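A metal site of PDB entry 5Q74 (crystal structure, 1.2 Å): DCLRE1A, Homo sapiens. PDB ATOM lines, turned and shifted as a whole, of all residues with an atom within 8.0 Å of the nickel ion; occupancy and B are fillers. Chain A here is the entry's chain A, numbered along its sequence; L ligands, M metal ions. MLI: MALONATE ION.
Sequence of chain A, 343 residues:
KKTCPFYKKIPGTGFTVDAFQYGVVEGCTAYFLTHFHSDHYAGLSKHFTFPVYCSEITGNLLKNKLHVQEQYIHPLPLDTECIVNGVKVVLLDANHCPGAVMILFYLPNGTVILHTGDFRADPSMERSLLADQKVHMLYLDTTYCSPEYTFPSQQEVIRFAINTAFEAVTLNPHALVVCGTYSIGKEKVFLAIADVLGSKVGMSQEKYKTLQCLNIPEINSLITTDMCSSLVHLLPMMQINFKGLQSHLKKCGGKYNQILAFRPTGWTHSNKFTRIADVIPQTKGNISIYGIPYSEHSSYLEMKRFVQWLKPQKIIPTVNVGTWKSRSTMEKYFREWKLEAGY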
ATOM      1  N   ASP A  18       7.351 -25.102 -12.948  1.00  0.00           N
ATOM      2  CA  ASP A  18       7.019 -26.412 -12.300  1.00  0.00           C
ATOM      3  C   ASP A  18       6.720 -27.540 -13.374  1.00  0.00           C
ATOM      4  O   ASP A  18       5.774 -28.321 -13.229  1.00  0.00           O
ATOM      5  CB  ASP A  18       5.956 -26.281 -11.256  1.00  0.00           C
ATOM      6  CG  ASP A  18       6.326 -25.274 -10.115  1.00  0.00           C
ATOM      7  OD1 ASP A  18       7.481 -24.925 -10.014  1.00  0.00           O
ATOM      8  OD2 ASP A  18       5.308 -24.941  -9.404  1.00  0.00           O
ATOM      9  N   THR A  34       8.902 -23.254  -8.249  1.00  0.00           N
ATOM     10  CA  THR A  34       8.292 -22.380  -7.203  1.00  0.00           C
ATOM     11  C   THR A  34       8.671 -22.852  -5.779  1.00  0.00           C
ATOM     12  O   THR A  34       8.832 -22.017  -4.874  1.00  0.00           O
ATOM     13  CB  THR A  34       6.820 -22.209  -7.350  1.00  0.00           C
ATOM     14  OG1 THR A  34       6.133 -23.483  -7.158  1.00  0.00           O
ATOM     15  CG2 THR A  34       6.425 -21.580  -8.667  1.00  0.00           C
ATOM     16  N   HIS A  35       8.720 -24.172  -5.559  1.00  0.00           N
ATOM     17  CA  HIS A  35       8.929 -24.752  -4.243  1.00  0.00           C
ATOM     18  C   HIS A  35       9.294 -26.222  -4.298  1.00  0.00           C
ATOM     19  O   HIS A  35       8.939 -26.901  -5.300  1.00  0.00           O
ATOM     20  CB  HIS A  35       7.755 -24.458  -3.260  1.00  0.00           C
ATOM     21  CG  HIS A  35       6.468 -25.141  -3.566  1.00  0.00           C
ATOM     22  ND1 HIS A  35       5.676 -24.941  -4.693  1.00  0.00           N
ATOM     23  CD2 HIS A  35       5.801 -26.092  -2.864  1.00  0.00           C
ATOM     24  CE1 HIS A  35       4.582 -25.674  -4.589  1.00  0.00           C
ATOM     25  NE2 HIS A  35       4.642 -26.389  -3.499  1.00  0.00           N
ATOM     26  N   PHE A  36       9.891 -26.693  -3.196  1.00  0.00           N
ATOM     27  CA  PHE A  36      10.309 -28.140  -3.119  1.00  0.00           C
ATOM     28  C   PHE A  36       9.225 -29.062  -2.599  1.00  0.00           C
ATOM     29  O   PHE A  36       9.374 -29.617  -1.462  1.00  0.00           O
ATOM     30  CB  PHE A  36      11.608 -28.204  -2.275  1.00  0.00           C
ATOM     31  CG  PHE A  36      12.373 -29.547  -2.401  1.00  0.00           C
ATOM     32  CD1 PHE A  36      13.142 -29.785  -3.537  1.00  0.00           C
ATOM     33  CD2 PHE A  36      12.355 -30.500  -1.392  1.00  0.00           C
ATOM     34  CE1 PHE A  36      13.862 -30.975  -3.669  1.00  0.00           C
ATOM     35  CE2 PHE A  36      13.083 -31.695  -1.520  1.00  0.00           C
ATOM     36  CZ  PHE A  36      13.822 -31.919  -2.620  1.00  0.00           C
ATOM     37  N   HIS A  37       8.135 -29.251  -3.348  1.00  0.00           N
ATOM     38  CA  HIS A  37       7.115 -30.275  -3.117  1.00  0.00           C
ATOM     39  C   HIS A  37       7.120 -31.212  -4.362  1.00  0.00           C
ATOM     40  O   HIS A  37       7.233 -30.755  -5.510  1.00  0.00           O
ATOM     41  CB  HIS A  37       5.711 -29.716  -2.859  1.00  0.00           C
ATOM     42  CG  HIS A  37       5.460 -29.236  -1.423  1.00  0.00           C
ATOM     43  ND1 HIS A  37       4.413 -28.413  -1.054  1.00  0.00           N
ATOM     44  CD2 HIS A  37       6.134 -29.511  -0.292  1.00  0.00           C
ATOM     45  CE1 HIS A  37       4.438 -28.220   0.261  1.00  0.00           C
ATOM     46  NE2 HIS A  37       5.493 -28.858   0.729  1.00  0.00           N
ATOM     47  N   SER A  38       6.942 -32.514  -4.105  1.00  0.00           N
ATOM     48  CA  SER A  38       7.149 -33.541  -5.163  1.00  0.00           C
ATOM     49  C   SER A  38       6.239 -33.405  -6.330  1.00  0.00           C
ATOM     50  O   SER A  38       6.765 -33.671  -7.442  1.00  0.00           O
ATOM     51  CB  SER A  38       7.212 -34.958  -4.552  1.00  0.00           C
ATOM     52  OG  SER A  38       5.977 -35.280  -3.958  1.00  0.00           O
ATOM     53  N   ASP A  39       4.994 -32.993  -6.206  1.00  0.00           N
ATOM     54  CA  ASP A  39       4.072 -32.821  -7.391  1.00  0.00           C
ATOM     55  C   ASP A  39       4.686 -31.735  -8.312  1.00  0.00           C
ATOM     56  O   ASP A  39       4.459 -31.790  -9.545  1.00  0.00           O
ATOM     57  CB  ASP A  39       2.648 -32.482  -7.008  1.00  0.00           C
ATOM     58  CG  ASP A  39       1.780 -33.729  -6.618  1.00  0.00           C
ATOM     59  OD1 ASP A  39       2.276 -34.866  -6.649  1.00  0.00           O
ATOM     60  OD2 ASP A  39       0.611 -33.473  -6.269  1.00  0.00           O
ATOM     61  N   HIS A  40       5.485 -30.785  -7.782  1.00  0.00           N
ATOM     62  CA  HIS A  40       6.024 -29.638  -8.556  1.00  0.00           C
ATOM     63  C   HIS A  40       7.384 -29.913  -9.059  1.00  0.00           C
ATOM     64  O   HIS A  40       7.739 -29.499 -10.222  1.00  0.00           O
ATOM     65  CB  HIS A  40       5.965 -28.356  -7.671  1.00  0.00           C
ATOM     66  CG  HIS A  40       4.588 -27.973  -7.330  1.00  0.00           C
ATOM     67  ND1 HIS A  40       3.870 -26.964  -7.933  1.00  0.00           N
ATOM     68  CD2 HIS A  40       3.762 -28.499  -6.406  1.00  0.00           C
ATOM     69  CE1 HIS A  40       2.648 -26.937  -7.444  1.00  0.00           C
ATOM     70  NE2 HIS A  40       2.569 -27.876  -6.499  1.00  0.00           N
ATOM     71  N   HIS A  96       3.828 -20.236   1.939  1.00  0.00           N
ATOM     72  CA  HIS A  96       3.515 -21.680   1.772  1.00  0.00           C
ATOM     73  C   HIS A  96       4.510 -22.421   2.635  1.00  0.00           C
ATOM     74  O   HIS A  96       4.427 -22.238   3.888  1.00  0.00           O
ATOM     75  CB  HIS A  96       3.489 -22.065   0.291  1.00  0.00           C
ATOM     76  CG  HIS A  96       3.085 -23.474  -0.081  1.00  0.00           C
ATOM     77  ND1 HIS A  96       1.932 -24.050   0.359  1.00  0.00           N
ATOM     78  CD2 HIS A  96       3.709 -24.404  -0.840  1.00  0.00           C
ATOM     79  CE1 HIS A  96       1.858 -25.291  -0.130  1.00  0.00           C
ATOM     80  NE2 HIS A  96       2.915 -25.538  -0.872  1.00  0.00           N
ATOM     81  N   CYS A  97       5.379 -23.236   2.135  1.00  0.00           N
ATOM     82  CA  CYS A  97       6.467 -23.938   2.896  1.00  0.00           C
ATOM     83  C   CYS A  97       7.768 -23.155   2.768  1.00  0.00           C
ATOM     84  O   CYS A  97       7.861 -22.176   1.988  1.00  0.00           O
ATOM     85  CB  CYS A  97       6.601 -25.367   2.310  1.00  0.00           C
ATOM     86  SG  CYS A  97       7.180 -25.434   0.569  1.00  0.00           S
ATOM     87  N   ALA A 100       9.280 -21.317  -0.632  1.00  0.00           N
ATOM     88  CA  ALA A 100       8.249 -21.198  -1.657  1.00  0.00           C
ATOM     89  C   ALA A 100       8.067 -19.751  -2.106  1.00  0.00           C
ATOM     90  O   ALA A 100       8.023 -18.837  -1.274  1.00  0.00           O
ATOM     91  CB  ALA A 100       6.950 -21.764  -1.185  1.00  0.00           C
ATOM     92  N   GLY A 117       2.525 -19.841  -7.723  1.00  0.00           N
ATOM     93  CA  GLY A 117       2.909 -21.189  -7.258  1.00  0.00           C
ATOM     94  C   GLY A 117       1.826 -21.693  -6.335  1.00  0.00           C
ATOM     95  O   GLY A 117       0.634 -21.469  -6.572  1.00  0.00           O
ATOM     96  N   ASP A 118       2.246 -22.435  -5.309  1.00  0.00           N
ATOM     97  CA  ASP A 118       1.338 -22.690  -4.152  1.00  0.00           C
ATOM     98  C   ASP A 118       1.454 -21.538  -3.121  1.00  0.00           C
ATOM     99  O   ASP A 118       2.603 -21.107  -2.815  1.00  0.00           O
ATOM    100  CB  ASP A 118       1.642 -24.025  -3.463  1.00  0.00           C
ATOM    101  CG  ASP A 118       1.142 -25.252  -4.192  1.00  0.00           C
ATOM    102  OD1 ASP A 118       0.377 -25.155  -5.174  1.00  0.00           O
ATOM    103  OD2 ASP A 118       1.457 -26.386  -3.747  1.00  0.00           O
ATOM    104  N   PHE A 119       0.343 -21.037  -2.604  1.00  0.00           N
ATOM    105  CA  PHE A 119       0.398 -19.895  -1.636  1.00  0.00           C
ATOM    106  C   PHE A 119      -0.763 -19.935  -0.659  1.00  0.00           C
ATOM    107  O   PHE A 119      -1.811 -20.520  -0.895  1.00  0.00           O
ATOM    108  CB  PHE A 119       0.521 -18.500  -2.368  1.00  0.00           C
ATOM    109  CG  PHE A 119      -0.785 -17.804  -2.868  1.00  0.00           C
ATOM    110  CD1 PHE A 119      -0.983 -16.429  -2.755  1.00  0.00           C
ATOM    111  CD2 PHE A 119      -1.836 -18.532  -3.479  1.00  0.00           C
ATOM    112  CE1 PHE A 119      -2.088 -15.783  -3.235  1.00  0.00           C
ATOM    113  CE2 PHE A 119      -3.011 -17.861  -3.928  1.00  0.00           C
ATOM    114  CZ  PHE A 119      -3.102 -16.504  -3.811  1.00  0.00           C
ATOM    115  N   ASP A 141      -3.183 -20.473  -7.574  1.00  0.00           N
ATOM    116  CA  ASP A 141      -3.365 -21.717  -6.724  1.00  0.00           C
ATOM    117  C   ASP A 141      -4.809 -21.671  -6.182  1.00  0.00           C
ATOM    118  O   ASP A 141      -5.197 -20.977  -5.259  1.00  0.00           O
ATOM    119  CB  ASP A 141      -2.396 -21.728  -5.563  1.00  0.00           C
ATOM    120  CG  ASP A 141      -2.691 -22.768  -4.510  1.00  0.00           C
ATOM    121  OD1 ASP A 141      -3.509 -23.671  -4.782  1.00  0.00           O
ATOM    122  OD2 ASP A 141      -2.092 -22.642  -3.406  1.00  0.00           O
ATOM    123  N   THR A 143      -6.488 -24.414  -4.936  1.00  0.00           N
ATOM    124  CA  THR A 143      -6.720 -25.672  -4.214  1.00  0.00           C
ATOM    125  C   THR A 143      -8.004 -25.629  -3.454  1.00  0.00           C
ATOM    126  O   THR A 143      -8.813 -26.641  -3.605  1.00  0.00           O
ATOM    127  CB  THR A 143      -5.514 -25.884  -3.210  1.00  0.00           C
ATOM    128  OG1 THR A 143      -4.278 -26.094  -3.889  1.00  0.00           O
ATOM    129  CG2 THR A 143      -5.752 -27.093  -2.354  1.00  0.00           C
ATOM    130  N   SER A 183       6.700 -34.166   3.970  1.00  0.00           N
ATOM    131  CA  SER A 183       7.219 -33.174   3.034  1.00  0.00           C
ATOM    132  C   SER A 183       7.725 -32.021   3.930  1.00  0.00           C
ATOM    133  O   SER A 183       7.430 -31.959   5.167  1.00  0.00           O
ATOM    134  CB  SER A 183       6.103 -32.636   2.090  1.00  0.00           C
ATOM    135  OG  SER A 183       5.041 -32.034   2.814  1.00  0.00           O
ATOM    136  N   ILE A 184       8.402 -31.068   3.354  1.00  0.00           N
ATOM    137  CA  ILE A 184       8.653 -29.788   4.038  1.00  0.00           C
ATOM    138  C   ILE A 184       7.369 -28.981   4.152  1.00  0.00           C
ATOM    139  O   ILE A 184       6.367 -29.239   3.426  1.00  0.00           O
ATOM    140  CB  ILE A 184       9.762 -28.913   3.395  1.00  0.00           C
ATOM    141  CG1 ILE A 184       9.390 -28.347   2.032  1.00  0.00           C
ATOM    142  CG2 ILE A 184      11.054 -29.680   3.335  1.00  0.00           C
ATOM    143  CD1 ILE A 184      10.324 -27.323   1.478  1.00  0.00           C
ATOM    144  N   GLU A 296      -1.345 -24.633   4.693  1.00  0.00           N
ATOM    145  CA  GLU A 296      -0.416 -23.744   3.932  1.00  0.00           C
ATOM    146  C   GLU A 296      -0.940 -23.291   2.529  1.00  0.00           C
ATOM    147  O   GLU A 296      -0.186 -22.846   1.667  1.00  0.00           O
ATOM    148  CB  GLU A 296       1.015 -24.285   3.898  1.00  0.00           C
ATOM    149  CG  GLU A 296       1.681 -24.224   5.326  1.00  0.00           C
ATOM    150  CD  GLU A 296       3.143 -24.678   5.377  1.00  0.00           C
ATOM    151  OE1 GLU A 296       3.666 -25.383   4.452  1.00  0.00           O
ATOM    152  OE2 GLU A 296       3.789 -24.341   6.427  1.00  0.00           O
ATOM    153  N   HIS A 297      -2.255 -23.484   2.361  1.00  0.00           N
ATOM    154  CA  HIS A 297      -2.995 -22.928   1.187  1.00  0.00           C
ATOM    155  C   HIS A 297      -4.104 -21.952   1.626  1.00  0.00           C
ATOM    156  O   HIS A 297      -4.668 -22.060   2.725  1.00  0.00           O
ATOM    157  CB  HIS A 297      -3.674 -24.064   0.369  1.00  0.00           C
ATOM    158  CG  HIS A 297      -2.745 -24.999  -0.309  1.00  0.00           C
ATOM    159  ND1 HIS A 297      -2.155 -24.777  -1.556  1.00  0.00           N
ATOM    160  CD2 HIS A 297      -2.342 -26.264   0.052  1.00  0.00           C
ATOM    161  CE1 HIS A 297      -1.431 -25.829  -1.899  1.00  0.00           C
ATOM    162  NE2 HIS A 297      -1.510 -26.715  -0.922  1.00  0.00           N
HETATM  163  C1  MLI L   1       1.473 -30.277  -1.879  1.00  0.00           C
HETATM  164  C2  MLI L   1       0.657 -29.166  -1.195  1.00  0.00           C
HETATM  165  C3  MLI L   1       1.932 -29.963  -3.308  1.00  0.00           C
HETATM  166  O6  MLI L   1      -0.426 -29.292  -0.614  1.00  0.00           O
HETATM  167  O7  MLI L   1       1.217 -28.074  -1.211  1.00  0.00           O
HETATM  168  O8  MLI L   1       2.639 -28.976  -3.557  1.00  0.00           O
HETATM  169  O9  MLI L   1       1.690 -30.807  -4.224  1.00  0.00           O
HETATM  170 NI    NI M   1       2.928 -27.278  -2.330  1.00  0.00          NI
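Four residues have an atom within 4 Å of the nickel ion: His 35, His 37, His 96 and Asp 118.
The side-chain hydroxyl of Thr 34 sits at hydrogen-bond distance from a ring nitrogen (ND1) of His 35 (2.9 Å).
The backbone carbonyl oxygen of Ile 184 is in hydrogen-bond range of a ring nitrogen (NE2) of His 37 (2.9 Å).
The side-chain carboxylate (OD2) of Asp 118 sits close to a ring nitrogen (NE2) of His 40, at 3.3 Å.
O of Glu 296 is in hydrogen-bond range of ND1 of His 96 (2.8 Å).
The nickel ion is bound by an oxygen (O8) of the ligand (2.1 Å).
The nickel ion is bound by an oxygen (O7) of the ligand (2.2 Å).
The side-chain carboxylate (OD2) of Asp 118 is bound to the nickel ion (2.2 Å).
The nickel ion is bound by a ring nitrogen (NE2) of His 35 (2.3 Å).
The nickel ion is bound by ND1 of His 37, 2.3 Å away.
The nickel ion is bound by NE2 of His 96 (2.3 Å).
The nickel ion has six donor atoms within binding distance.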
